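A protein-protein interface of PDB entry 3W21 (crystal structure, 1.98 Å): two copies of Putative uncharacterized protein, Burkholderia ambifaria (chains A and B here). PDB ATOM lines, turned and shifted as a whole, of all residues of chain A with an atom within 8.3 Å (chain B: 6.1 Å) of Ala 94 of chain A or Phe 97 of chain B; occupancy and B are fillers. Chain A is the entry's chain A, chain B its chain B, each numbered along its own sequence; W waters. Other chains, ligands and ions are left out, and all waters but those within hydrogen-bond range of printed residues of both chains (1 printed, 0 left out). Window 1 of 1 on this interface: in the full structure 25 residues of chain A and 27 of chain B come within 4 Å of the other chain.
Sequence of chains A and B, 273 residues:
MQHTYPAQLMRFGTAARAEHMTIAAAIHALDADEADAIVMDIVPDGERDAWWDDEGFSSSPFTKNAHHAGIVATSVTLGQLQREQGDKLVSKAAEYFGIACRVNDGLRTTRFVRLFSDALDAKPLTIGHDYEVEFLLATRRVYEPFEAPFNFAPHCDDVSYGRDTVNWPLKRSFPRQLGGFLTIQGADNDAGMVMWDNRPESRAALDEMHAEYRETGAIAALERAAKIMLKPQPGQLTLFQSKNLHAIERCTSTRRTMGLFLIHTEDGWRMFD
The side-chain sulfur (SG) of Cys 101 of chain A sits at hydrogen-bond distance from the backbone NH (N) of Arg 102 of chain B (3.8 Å).
SG of Cys 101 of chain B forms a disulfide with SG of Cys 101 of chain A.
The side-chain sulfur (SG) of Cys 101 of chain B sits close to the backbone carbonyl oxygen (O) of Gly 98 of chain A (3.1 Å).
NH2 of Arg 102 of chain A sits at hydrogen-bond distance from O of Cys 101 of chain B, at 3.4 Å.
OE1 of Glu 95 of chain B is in salt-bridge range of NZ of Lys 92 of chain B, at 3.4 Å.
O of Val 133 of chain B sits at hydrogen-bond distance from N of Ile 127 of chain B, at 2.8 Å.
The side-chain amino group of Lys 92 of chain A lies within salt-bridge range of the side-chain carboxylate of Glu 95 of chain A.
Ala 93 of chain B touches Val 90 of chain A.
Ile 127 of chain B touches Ser 91 of chain A (CD1 to OG, 3.7 Å).
Ala 94 of chain A touches Phe 97 of chain B.
CB of Ala 94 of chain A touches CG2 of Ile 127 of chain B, at 3.6 Å.
Ala 94 of chain A touches Val 133 of chain B.
Val 133 of chain B touches Glu 95 of chain A (CG1 to O, 3.9 Å).
CB of Ala 94 of chain B touches CD2 of Phe 97 of chain A (3.4 Å).
Gly 98 of chain A touches Phe 97 of chain B.
Val 133 of chain B touches Ile 99 of chain A.
Val 133 of chain A touches Ala 94 of chain B (CG2 to O, 3.5 Å).
Printed residues of chain B within 4 Å of Val 90 of chain A: Ala 93.
Of the printed residues of chain B, Ser 91 of chain A touches Ile 127 (3.7 Å).
Ala 94 of chain A touches just these residues of chain B: Phe 97 (3.3 Å), Ile 127 (3.6 Å) and Val 133 (3.4 Å).
Phe 97 of chain B touches two residues of chain A.
Of chain A, only Val 133 (3.9 Å) comes within 4 Å of Gly 98 of chain B.
The nearest residue of chain B that does not touch Ala 94 of chain A is Ala 93 of chain B (5.0 Å).
The nearest residue of chain A that does not touch Phe 97 of chain B is Phe 97 of chain A (4.7 Å).
The nearest printed residue of chain B that does not touch Val 133 of chain A is Ile 99 of chain B (4.02 Å).
Of the 19 printed residues of chain A, 10 touch a printed residue of chain B.
Hydrophobic or aromatic side chains of chain A that line the printed part of chain B: Val 90, Ala 94, Phe 97, Ile 99 and Val 133.
Printed residues of chain B that touch a printed residue of chain A: Ala 93, Ala 94, Glu 95, Phe 97, Gly 98, Cys 101, Arg 102, Ile 127 and Val 133.
Hydrophobic or aromatic side chains of chain B that line the printed part of chain A: Ala 93, Ala 94, Phe 97, Ile 127 and Val 133.
Among the printed residues, 17 pairs touch across the chains.
Among the printed residues, no Asp or Glu carboxylate lies within 4 Å of a Lys or Arg side-chain nitrogen of the other chain.
Glu 95 of chain A touches Val 133 of chain B, and with the chains exchanged Val 133 of chain A touches Glu 95 of chain B.
Gly 98 of chain A touches Val 133 of chain B, and with the chains exchanged Val 133 of chain A touches Gly 98 of chain B.
Ile 99 of chain A touches Val 133 of chain B, but with the chains exchanged Val 133 of chain A does not touch Ile 99 of chain B (4.02 Å).
Cys 101 of chain A touches Arg 102 of chain B, and with the chains exchanged Arg 102 of chain A touches Cys 101 of chain B.
Water W1 lies within hydrogen-bond range of the backbone carbonyl oxygen of Gly 98 of chain A (2.7 Å), the guanidinium group of Arg 102 of chain A (3.3 Å) and the side-chain sulfur of Cys 101 of chain B (3.5 Å).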
ATOM      1  N   VAL A  76       9.751 -37.875  28.633  1.00  0.00           N
ATOM      2  CA  VAL A  76       9.138 -37.757  27.301  1.00  0.00           C
ATOM      3  C   VAL A  76      10.017 -38.553  26.329  1.00  0.00           C
ATOM      4  O   VAL A  76      11.231 -38.468  26.386  1.00  0.00           O
ATOM      5  CB  VAL A  76       9.068 -36.278  26.878  1.00  0.00           C
ATOM      6  CG1 VAL A  76       8.334 -36.091  25.539  1.00  0.00           C
ATOM      7  CG2 VAL A  76       8.425 -35.444  27.983  1.00  0.00           C
ATOM      8  N   LEU A  81       7.079 -37.225  21.560  1.00  0.00           N
ATOM      9  CA  LEU A  81       7.338 -35.978  20.925  1.00  0.00           C
ATOM     10  C   LEU A  81       6.778 -35.926  19.490  1.00  0.00           C
ATOM     11  O   LEU A  81       6.136 -34.920  19.086  1.00  0.00           O
ATOM     12  CB  LEU A  81       8.854 -35.604  21.029  1.00  0.00           C
ATOM     13  CG  LEU A  81       9.248 -34.260  20.375  1.00  0.00           C
ATOM     14  CD1 LEU A  81       8.561 -33.088  21.057  1.00  0.00           C
ATOM     15  CD2 LEU A  81      10.745 -34.072  20.410  1.00  0.00           C
ATOM     16  N   ASP A  87       2.061 -25.532  18.025  1.00  0.00           N
ATOM     17  CA  ASP A  87       2.635 -24.939  19.239  1.00  0.00           C
ATOM     18  C   ASP A  87       2.829 -25.968  20.303  1.00  0.00           C
ATOM     19  O   ASP A  87       3.725 -25.831  21.180  1.00  0.00           O
ATOM     20  CB  ASP A  87       1.860 -23.711  19.785  1.00  0.00           C
ATOM     21  CG  ASP A  87       0.475 -24.069  20.338  1.00  0.00           C
ATOM     22  OD1 ASP A  87      -0.280 -24.845  19.707  1.00  0.00           O
ATOM     23  OD2 ASP A  87       0.137 -23.560  21.416  1.00  0.00           O
ATOM     24  N   LYS A  88       2.018 -27.009  20.284  1.00  0.00           N
ATOM     25  CA  LYS A  88       2.278 -28.041  21.297  1.00  0.00           C
ATOM     26  C   LYS A  88       3.577 -28.843  20.983  1.00  0.00           C
ATOM     27  O   LYS A  88       4.186 -29.404  21.898  1.00  0.00           O
ATOM     28  CB  LYS A  88       1.097 -28.961  21.500  1.00  0.00           C
ATOM     29  CG  LYS A  88      -0.138 -28.240  22.070  1.00  0.00           C
ATOM     30  CD  LYS A  88      -1.326 -29.081  21.657  1.00  0.00           C
ATOM     31  CE  LYS A  88      -2.625 -28.576  22.272  1.00  0.00           C
ATOM     32  NZ  LYS A  88      -3.719 -28.985  21.342  1.00  0.00           N
ATOM     33  N   LEU A  89       3.964 -28.908  19.702  1.00  0.00           N
ATOM     34  CA  LEU A  89       5.276 -29.446  19.364  1.00  0.00           C
ATOM     35  C   LEU A  89       6.454 -28.611  19.881  1.00  0.00           C
ATOM     36  O   LEU A  89       7.403 -29.182  20.456  1.00  0.00           O
ATOM     37  CB  LEU A  89       5.435 -29.737  17.870  1.00  0.00           C
ATOM     38  CG  LEU A  89       6.747 -30.228  17.245  1.00  0.00           C
ATOM     39  CD1 LEU A  89       7.083 -31.637  17.765  1.00  0.00           C
ATOM     40  CD2 LEU A  89       6.613 -30.226  15.702  1.00  0.00           C
ATOM     41  N   VAL A  90       6.421 -27.288  19.668  1.00  0.00           N
ATOM     42  CA  VAL A  90       7.482 -26.428  20.233  1.00  0.00           C
ATOM     43  C   VAL A  90       7.601 -26.610  21.749  1.00  0.00           C
ATOM     44  O   VAL A  90       8.681 -26.866  22.295  1.00  0.00           O
ATOM     45  CB  VAL A  90       7.237 -24.994  19.923  1.00  0.00           C
ATOM     46  CG1 VAL A  90       8.408 -24.160  20.438  1.00  0.00           C
ATOM     47  CG2 VAL A  90       7.019 -24.876  18.392  1.00  0.00           C
ATOM     48  N   SER A  91       6.451 -26.592  22.408  1.00  0.00           N
ATOM     49  CA  SER A  91       6.361 -26.838  23.843  1.00  0.00           C
ATOM     50  C   SER A  91       6.912 -28.211  24.273  1.00  0.00           C
ATOM     51  O   SER A  91       7.724 -28.283  25.185  1.00  0.00           O
ATOM     52  CB  SER A  91       4.877 -26.728  24.244  1.00  0.00           C
ATOM     53  OG  SER A  91       4.817 -26.489  25.626  1.00  0.00           O
ATOM     54  N   LYS A  92       6.421 -29.316  23.693  1.00  0.00           N
ATOM     55  CA  LYS A  92       6.897 -30.677  24.110  1.00  0.00           C
ATOM     56  C   LYS A  92       8.396 -30.818  23.799  1.00  0.00           C
ATOM     57  O   LYS A  92       9.079 -31.535  24.484  1.00  0.00           O
ATOM     58  CB  LYS A  92       6.077 -31.761  23.407  1.00  0.00           C
ATOM     59  CG  LYS A  92       6.182 -33.174  23.946  1.00  0.00           C
ATOM     60  CD  LYS A  92       5.966 -33.280  25.460  1.00  0.00           C
ATOM     61  CE  LYS A  92       4.499 -33.360  25.882  1.00  0.00           C
ATOM     62  NZ  LYS A  92       4.400 -33.056  27.338  1.00  0.00           N
ATOM     63  N   ALA A  93       8.884 -30.174  22.730  1.00  0.00           N
ATOM     64  CA  ALA A  93      10.308 -30.325  22.391  1.00  0.00           C
ATOM     65  C   ALA A  93      11.100 -29.625  23.511  1.00  0.00           C
ATOM     66  O   ALA A  93      12.142 -30.122  23.898  1.00  0.00           O
ATOM     67  CB  ALA A  93      10.639 -29.708  21.021  1.00  0.00           C
ATOM     68  N   ALA A  94      10.595 -28.495  24.060  1.00  0.00           N
ATOM     69  CA  ALA A  94      11.326 -27.806  25.162  1.00  0.00           C
ATOM     70  C   ALA A  94      11.439 -28.810  26.306  1.00  0.00           C
ATOM     71  O   ALA A  94      12.487 -29.037  26.892  1.00  0.00           O
ATOM     72  CB  ALA A  94      10.559 -26.564  25.655  1.00  0.00           C
ATOM     73  N   GLU A  95      10.341 -29.458  26.609  1.00  0.00           N
ATOM     74  CA  GLU A  95      10.344 -30.435  27.647  1.00  0.00           C
ATOM     75  C   GLU A  95      11.289 -31.571  27.385  1.00  0.00           C
ATOM     76  O   GLU A  95      12.096 -31.934  28.273  1.00  0.00           O
ATOM     77  CB  GLU A  95       8.972 -31.027  27.777  1.00  0.00           C
ATOM     78  CG  GLU A  95       8.218 -30.465  28.915  1.00  0.00           C
ATOM     79  CD  GLU A  95       6.847 -31.065  28.929  1.00  0.00           C
ATOM     80  OE1 GLU A  95       6.029 -30.465  28.242  1.00  0.00           O
ATOM     81  OE2 GLU A  95       6.641 -32.164  29.528  1.00  0.00           O
ATOM     82  N   TYR A  96      11.249 -32.071  26.156  1.00  0.00           N
ATOM     83  CA  TYR A  96      12.065 -33.223  25.767  1.00  0.00           C
ATOM     84  C   TYR A  96      13.536 -32.953  25.874  1.00  0.00           C
ATOM     85  O   TYR A  96      14.244 -33.733  26.541  1.00  0.00           O
ATOM     86  CB  TYR A  96      11.719 -33.708  24.352  1.00  0.00           C
ATOM     87  CG  TYR A  96      12.576 -34.932  23.905  1.00  0.00           C
ATOM     88  CD1 TYR A  96      12.236 -36.249  24.227  1.00  0.00           C
ATOM     89  CD2 TYR A  96      13.725 -34.736  23.124  1.00  0.00           C
ATOM     90  CE1 TYR A  96      13.031 -37.347  23.758  1.00  0.00           C
ATOM     91  CE2 TYR A  96      14.514 -35.799  22.663  1.00  0.00           C
ATOM     92  CZ  TYR A  96      14.142 -37.093  22.965  1.00  0.00           C
ATOM     93  OH  TYR A  96      14.942 -38.079  22.499  1.00  0.00           O
ATOM     94  N   PHE A  97      14.006 -31.877  25.237  1.00  0.00           N
ATOM     95  CA  PHE A  97      15.430 -31.545  25.250  1.00  0.00           C
ATOM     96  C   PHE A  97      15.874 -30.960  26.604  1.00  0.00           C
ATOM     97  O   PHE A  97      16.982 -31.168  27.029  1.00  0.00           O
ATOM     98  CB  PHE A  97      15.838 -30.680  24.054  1.00  0.00           C
ATOM     99  CG  PHE A  97      15.729 -31.435  22.727  1.00  0.00           C
ATOM    100  CD1 PHE A  97      16.772 -32.280  22.305  1.00  0.00           C
ATOM    101  CD2 PHE A  97      14.536 -31.401  21.976  1.00  0.00           C
ATOM    102  CE1 PHE A  97      16.676 -33.042  21.152  1.00  0.00           C
ATOM    103  CE2 PHE A  97      14.438 -32.164  20.796  1.00  0.00           C
ATOM    104  CZ  PHE A  97      15.510 -32.990  20.410  1.00  0.00           C
ATOM    105  N   GLY A  98      14.988 -30.240  27.294  1.00  0.00           N
ATOM    106  CA  GLY A  98      15.351 -29.738  28.607  1.00  0.00           C
ATOM    107  C   GLY A  98      15.542 -30.883  29.582  1.00  0.00           C
ATOM    108  O   GLY A  98      16.422 -30.843  30.449  1.00  0.00           O
ATOM    109  N   ILE A  99      14.764 -31.937  29.431  1.00  0.00           N
ATOM    110  CA  ILE A  99      14.837 -33.085  30.338  1.00  0.00           C
ATOM    111  C   ILE A  99      16.051 -33.977  30.042  1.00  0.00           C
ATOM    112  O   ILE A  99      16.779 -34.353  30.961  1.00  0.00           O
ATOM    113  CB  ILE A  99      13.526 -33.913  30.363  1.00  0.00           C
ATOM    114  CG1 ILE A  99      12.449 -33.204  31.234  1.00  0.00           C
ATOM    115  CG2 ILE A  99      13.727 -35.337  30.843  1.00  0.00           C
ATOM    116  CD1 ILE A  99      12.973 -32.491  32.486  1.00  0.00           C
ATOM    117  N   ALA A 100      16.268 -34.278  28.764  1.00  0.00           N
ATOM    118  CA  ALA A 100      17.360 -35.126  28.318  1.00  0.00           C
ATOM    119  C   ALA A 100      18.678 -34.749  29.001  1.00  0.00           C
ATOM    120  O   ALA A 100      19.449 -35.615  29.390  1.00  0.00           O
ATOM    121  CB  ALA A 100      17.500 -35.074  26.796  1.00  0.00           C
ATOM    122  N   CYS A 101      18.967 -33.453  29.096  1.00  0.00           N
ATOM    123  CA  CYS A 101      20.266 -33.049  29.629  1.00  0.00           C
ATOM    124  C   CYS A 101      20.347 -33.384  31.121  1.00  0.00           C
ATOM    125  O   CYS A 101      21.407 -33.783  31.568  1.00  0.00           O
ATOM    126  CB  CYS A 101      20.611 -31.597  29.266  1.00  0.00           C
ATOM    127  SG  CYS A 101      21.027 -30.502  30.663  1.00  0.00           S
ATOM    128  N   ARG A 102      19.242 -33.285  31.874  1.00  0.00           N
ATOM    129  CA  ARG A 102      19.253 -33.709  33.302  1.00  0.00           C
ATOM    130  C   ARG A 102      19.492 -35.190  33.461  1.00  0.00           C
ATOM    131  O   ARG A 102      20.150 -35.637  34.391  1.00  0.00           O
ATOM    132  CB  ARG A 102      17.925 -33.386  34.023  1.00  0.00           C
ATOM    133  CG  ARG A 102      17.614 -31.897  34.166  1.00  0.00           C
ATOM    134  CD  ARG A 102      18.162 -31.202  35.423  1.00  0.00           C
ATOM    135  NE  ARG A 102      18.291 -29.734  35.262  1.00  0.00           N
ATOM    136  CZ  ARG A 102      19.406 -29.027  35.497  1.00  0.00           C
ATOM    137  NH1 ARG A 102      20.513 -29.647  35.921  1.00  0.00           N
ATOM    138  NH2 ARG A 102      19.429 -27.692  35.322  1.00  0.00           N
ATOM    139  N   VAL A 133      22.921 -30.303  21.358  1.00  0.00           N
ATOM    140  CA  VAL A 133      22.223 -30.700  22.584  1.00  0.00           C
ATOM    141  C   VAL A 133      21.755 -32.120  22.379  1.00  0.00           C
ATOM    142  O   VAL A 133      21.491 -32.486  21.256  1.00  0.00           O
ATOM    143  CB  VAL A 133      21.114 -29.709  23.007  1.00  0.00           C
ATOM    144  CG1 VAL A 133      21.610 -28.246  22.958  1.00  0.00           C
ATOM    145  CG2 VAL A 133      19.871 -29.926  22.234  1.00  0.00           C
ATOM    146  N   LEU B  78      16.069 -15.811  23.824  1.00  0.00           N
ATOM    147  CA  LEU B  78      14.646 -15.855  23.512  1.00  0.00           C
ATOM    148  C   LEU B  78      14.281 -14.984  22.317  1.00  0.00           C
ATOM    149  O   LEU B  78      13.457 -15.405  21.475  1.00  0.00           O
ATOM    150  CB  LEU B  78      13.769 -15.601  24.765  1.00  0.00           C
ATOM    151  CG  LEU B  78      12.290 -15.791  24.430  1.00  0.00           C
ATOM    152  CD1 LEU B  78      11.912 -17.262  24.351  1.00  0.00           C
ATOM    153  CD2 LEU B  78      11.454 -15.122  25.482  1.00  0.00           C
ATOM    154  N   LEU B  81      15.150 -16.896  19.299  1.00  0.00           N
ATOM    155  CA  LEU B  81      14.313 -18.025  19.172  1.00  0.00           C
ATOM    156  C   LEU B  81      12.995 -17.569  18.528  1.00  0.00           C
ATOM    157  O   LEU B  81      12.460 -18.204  17.584  1.00  0.00           O
ATOM    158  CB  LEU B  81      14.072 -18.713  20.553  1.00  0.00           C
ATOM    159  CG  LEU B  81      13.171 -19.929  20.477  1.00  0.00           C
ATOM    160  CD1 LEU B  81      13.781 -21.088  19.569  1.00  0.00           C
ATOM    161  CD2 LEU B  81      12.917 -20.389  21.888  1.00  0.00           C
ATOM    162  N   LYS B  92      15.477 -24.877  16.818  1.00  0.00           N
ATOM    163  CA  LYS B  92      16.125 -23.840  17.607  1.00  0.00           C
ATOM    164  C   LYS B  92      15.601 -23.859  19.036  1.00  0.00           C
ATOM    165  O   LYS B  92      16.309 -23.517  19.942  1.00  0.00           O
ATOM    166  CB  LYS B  92      15.968 -22.448  16.984  1.00  0.00           C
ATOM    167  CG  LYS B  92      17.163 -21.536  17.213  1.00  0.00           C
ATOM    168  CD  LYS B  92      18.245 -21.714  16.122  1.00  0.00           C
ATOM    169  CE  LYS B  92      19.274 -20.612  16.254  1.00  0.00           C
ATOM    170  NZ  LYS B  92      20.661 -21.125  16.401  1.00  0.00           N
ATOM    171  N   ALA B  93      14.374 -24.292  19.230  1.00  0.00           N
ATOM    172  CA  ALA B  93      13.843 -24.442  20.617  1.00  0.00           C
ATOM    173  C   ALA B  93      14.571 -25.585  21.307  1.00  0.00           C
ATOM    174  O   ALA B  93      14.936 -25.499  22.491  1.00  0.00           O
ATOM    175  CB  ALA B  93      12.362 -24.699  20.589  1.00  0.00           C
ATOM    176  N   ALA B  94      14.828 -26.660  20.570  1.00  0.00           N
ATOM    177  CA  ALA B  94      15.563 -27.788  21.162  1.00  0.00           C
ATOM    178  C   ALA B  94      16.901 -27.264  21.659  1.00  0.00           C
ATOM    179  O   ALA B  94      17.304 -27.539  22.778  1.00  0.00           O
ATOM    180  CB  ALA B  94      15.788 -28.892  20.125  1.00  0.00           C
ATOM    181  N   GLU B  95      17.585 -26.494  20.834  1.00  0.00           N
ATOM    182  CA  GLU B  95      18.874 -25.944  21.194  1.00  0.00           C
ATOM    183  C   GLU B  95      18.784 -24.988  22.372  1.00  0.00           C
ATOM    184  O   GLU B  95      19.668 -25.027  23.234  1.00  0.00           O
ATOM    185  CB  GLU B  95      19.490 -25.153  20.038  1.00  0.00           C
ATOM    186  CG  GLU B  95      20.059 -25.987  18.917  1.00  0.00           C
ATOM    187  CD  GLU B  95      20.646 -25.072  17.882  1.00  0.00           C
ATOM    188  OE1 GLU B  95      19.854 -24.377  17.201  1.00  0.00           O
ATOM    189  OE2 GLU B  95      21.890 -24.996  17.815  1.00  0.00           O
ATOM    190  N   TYR B  96      17.792 -24.081  22.350  1.00  0.00           N
ATOM    191  CA  TYR B  96      17.628 -23.065  23.410  1.00  0.00           C
ATOM    192  C   TYR B  96      17.387 -23.717  24.797  1.00  0.00           C
ATOM    193  O   TYR B  96      18.077 -23.414  25.777  1.00  0.00           O
ATOM    194  CB  TYR B  96      16.432 -22.121  23.089  1.00  0.00           C
ATOM    195  CG  TYR B  96      16.137 -21.099  24.228  1.00  0.00           C
ATOM    196  CD1 TYR B  96      16.873 -19.912  24.345  1.00  0.00           C
ATOM    197  CD2 TYR B  96      15.076 -21.299  25.133  1.00  0.00           C
ATOM    198  CE1 TYR B  96      16.590 -18.970  25.335  1.00  0.00           C
ATOM    199  CE2 TYR B  96      14.791 -20.353  26.113  1.00  0.00           C
ATOM    200  CZ  TYR B  96      15.550 -19.215  26.219  1.00  0.00           C
ATOM    201  OH  TYR B  96      15.262 -18.324  27.234  1.00  0.00           O
ATOM    202  N   PHE B  97      16.451 -24.648  24.866  1.00  0.00           N
ATOM    203  CA  PHE B  97      16.172 -25.339  26.106  1.00  0.00           C
ATOM    204  C   PHE B  97      17.247 -26.345  26.546  1.00  0.00           C
ATOM    205  O   PHE B  97      17.476 -26.534  27.769  1.00  0.00           O
ATOM    206  CB  PHE B  97      14.779 -25.957  26.075  1.00  0.00           C
ATOM    207  CG  PHE B  97      13.707 -24.931  26.104  1.00  0.00           C
ATOM    208  CD1 PHE B  97      13.392 -24.271  27.315  1.00  0.00           C
ATOM    209  CD2 PHE B  97      13.075 -24.522  24.930  1.00  0.00           C
ATOM    210  CE1 PHE B  97      12.425 -23.262  27.354  1.00  0.00           C
ATOM    211  CE2 PHE B  97      12.074 -23.542  24.984  1.00  0.00           C
ATOM    212  CZ  PHE B  97      11.749 -22.914  26.192  1.00  0.00           C
ATOM    213  N   GLY B  98      17.899 -26.971  25.572  1.00  0.00           N
ATOM    214  CA  GLY B  98      19.084 -27.827  25.871  1.00  0.00           C
ATOM    215  C   GLY B  98      20.264 -27.044  26.475  1.00  0.00           C
ATOM    216  O   GLY B  98      20.944 -27.510  27.418  1.00  0.00           O
ATOM    217  N   ILE B  99      20.502 -25.842  25.988  1.00  0.00           N
ATOM    218  CA  ILE B  99      21.582 -24.995  26.525  1.00  0.00           C
ATOM    219  C   ILE B  99      21.214 -24.530  27.913  1.00  0.00           C
ATOM    220  O   ILE B  99      22.043 -24.533  28.821  1.00  0.00           O
ATOM    221  CB  ILE B  99      21.855 -23.792  25.607  1.00  0.00           C
ATOM    222  CG1 ILE B  99      22.456 -24.254  24.274  1.00  0.00           C
ATOM    223  CG2 ILE B  99      22.715 -22.692  26.263  1.00  0.00           C
ATOM    224  CD1 ILE B  99      23.745 -25.031  24.385  1.00  0.00           C
ATOM    225  N   ALA B 100      19.959 -24.115  28.071  1.00  0.00           N
ATOM    226  CA  ALA B 100      19.506 -23.619  29.362  1.00  0.00           C
ATOM    227  C   ALA B 100      19.684 -24.682  30.446  1.00  0.00           C
ATOM    228  O   ALA B 100      20.112 -24.339  31.552  1.00  0.00           O
ATOM    229  CB  ALA B 100      18.077 -23.147  29.287  1.00  0.00           C
ATOM    230  N   CYS B 101      19.371 -25.932  30.110  1.00  0.00           N
ATOM    231  CA  CYS B 101      19.584 -27.071  30.994  1.00  0.00           C
ATOM    232  C   CYS B 101      21.076 -27.136  31.381  1.00  0.00           C
ATOM    233  O   CYS B 101      21.370 -27.329  32.549  1.00  0.00           O
ATOM    234  CB  CYS B 101      19.019 -28.370  30.380  1.00  0.00           C
ATOM    235  SG  CYS B 101      19.227 -29.908  31.366  1.00  0.00           S
ATOM    236  N   ARG B 102      21.986 -26.840  30.448  1.00  0.00           N
ATOM    237  CA  ARG B 102      23.440 -26.940  30.674  1.00  0.00           C
ATOM    238  C   ARG B 102      23.977 -25.805  31.554  1.00  0.00           C
ATOM    239  O   ARG B 102      24.729 -26.055  32.466  1.00  0.00           O
ATOM    240  CB  ARG B 102      24.219 -26.995  29.351  1.00  0.00           C
ATOM    241  N   ILE B 127       8.634 -23.770  31.366  1.00  0.00           N
ATOM    242  CA  ILE B 127       7.600 -24.153  30.395  1.00  0.00           C
ATOM    243  C   ILE B 127       7.309 -25.628  30.613  1.00  0.00           C
ATOM    244  O   ILE B 127       8.180 -26.364  31.106  1.00  0.00           O
ATOM    245  CB  ILE B 127       7.984 -23.822  28.919  1.00  0.00           C
ATOM    246  CG1 ILE B 127       6.717 -23.892  28.048  1.00  0.00           C
ATOM    247  CG2 ILE B 127       9.154 -24.691  28.416  1.00  0.00           C
ATOM    248  CD1 ILE B 127       6.892 -23.632  26.577  1.00  0.00           C
ATOM    249  N   VAL B 133      10.589 -27.257  32.488  1.00  0.00           N
ATOM    250  CA  VAL B 133      11.968 -26.994  32.143  1.00  0.00           C
ATOM    251  C   VAL B 133      12.196 -25.484  32.061  1.00  0.00           C
ATOM    252  O   VAL B 133      11.268 -24.706  31.825  1.00  0.00           O
ATOM    253  CB  VAL B 133      12.425 -27.722  30.877  1.00  0.00           C
ATOM    254  CG1 VAL B 133      12.238 -29.222  31.026  1.00  0.00           C
ATOM    255  CG2 VAL B 133      11.734 -27.218  29.620  1.00  0.00           C
ATOM    256  N   GLU B 134      13.428 -25.087  32.324  1.00  0.00           N
ATOM    257  CA  GLU B 134      13.817 -23.684  32.455  1.00  0.00           C
ATOM    258  C   GLU B 134      14.126 -22.992  31.122  1.00  0.00           C
ATOM    259  O   GLU B 134      14.729 -23.599  30.234  1.00  0.00           O
ATOM    260  CB  GLU B 134      15.045 -23.655  33.387  1.00  0.00           C
ATOM    261  CG  GLU B 134      14.619 -23.955  34.818  1.00  0.00           C
ATOM    262  CD  GLU B 134      15.781 -23.947  35.777  1.00  0.00           C
ATOM    263  OE1 GLU B 134      16.877 -23.690  35.288  1.00  0.00           O
ATOM    264  OE2 GLU B 134      15.550 -24.119  37.002  1.00  0.00           O
ATOM    265  N   PHE B 135      13.708 -21.723  30.990  1.00  0.00           N
ATOM    266  CA  PHE B 135      14.309 -20.810  30.019  1.00  0.00           C
ATOM    267  C   PHE B 135      15.722 -20.449  30.487  1.00  0.00           C
ATOM    268  O   PHE B 135      16.085 -20.585  31.648  1.00  0.00           O
ATOM    269  CB  PHE B 135      13.492 -19.510  29.907  1.00  0.00           C
ATOM    270  CG  PHE B 135      12.144 -19.705  29.277  1.00  0.00           C
ATOM    271  CD1 PHE B 135      11.870 -19.111  28.060  1.00  0.00           C
ATOM    272  CD2 PHE B 135      11.150 -20.495  29.894  1.00  0.00           C
ATOM    273  CE1 PHE B 135      10.616 -19.260  27.461  1.00  0.00           C
ATOM    274  CE2 PHE B 135       9.893 -20.661  29.302  1.00  0.00           C
ATOM    275  CZ  PHE B 135       9.628 -20.030  28.081  1.00  0.00           C
ATOM    276  N   LEU B 136      16.527 -19.995  29.559  1.00  0.00           N
ATOM    277  CA  LEU B 136      17.804 -19.455  29.831  1.00  0.00           C
ATOM    278  C   LEU B 136      17.674 -18.243  30.760  1.00  0.00           C
ATOM    279  O   LEU B 136      16.803 -17.371  30.595  1.00  0.00           O
ATOM    280  CB  LEU B 136      18.435 -19.016  28.542  1.00  0.00           C
ATOM    281  CG  LEU B 136      19.863 -18.478  28.652  1.00  0.00           C
ATOM    282  CD1 LEU B 136      20.871 -19.543  29.121  1.00  0.00           C
ATOM    283  CD2 LEU B 136      20.317 -17.847  27.331  1.00  0.00           C
HETATM  284  O   HOH W   1      16.021 -29.646  32.860  1.00  0.00           O
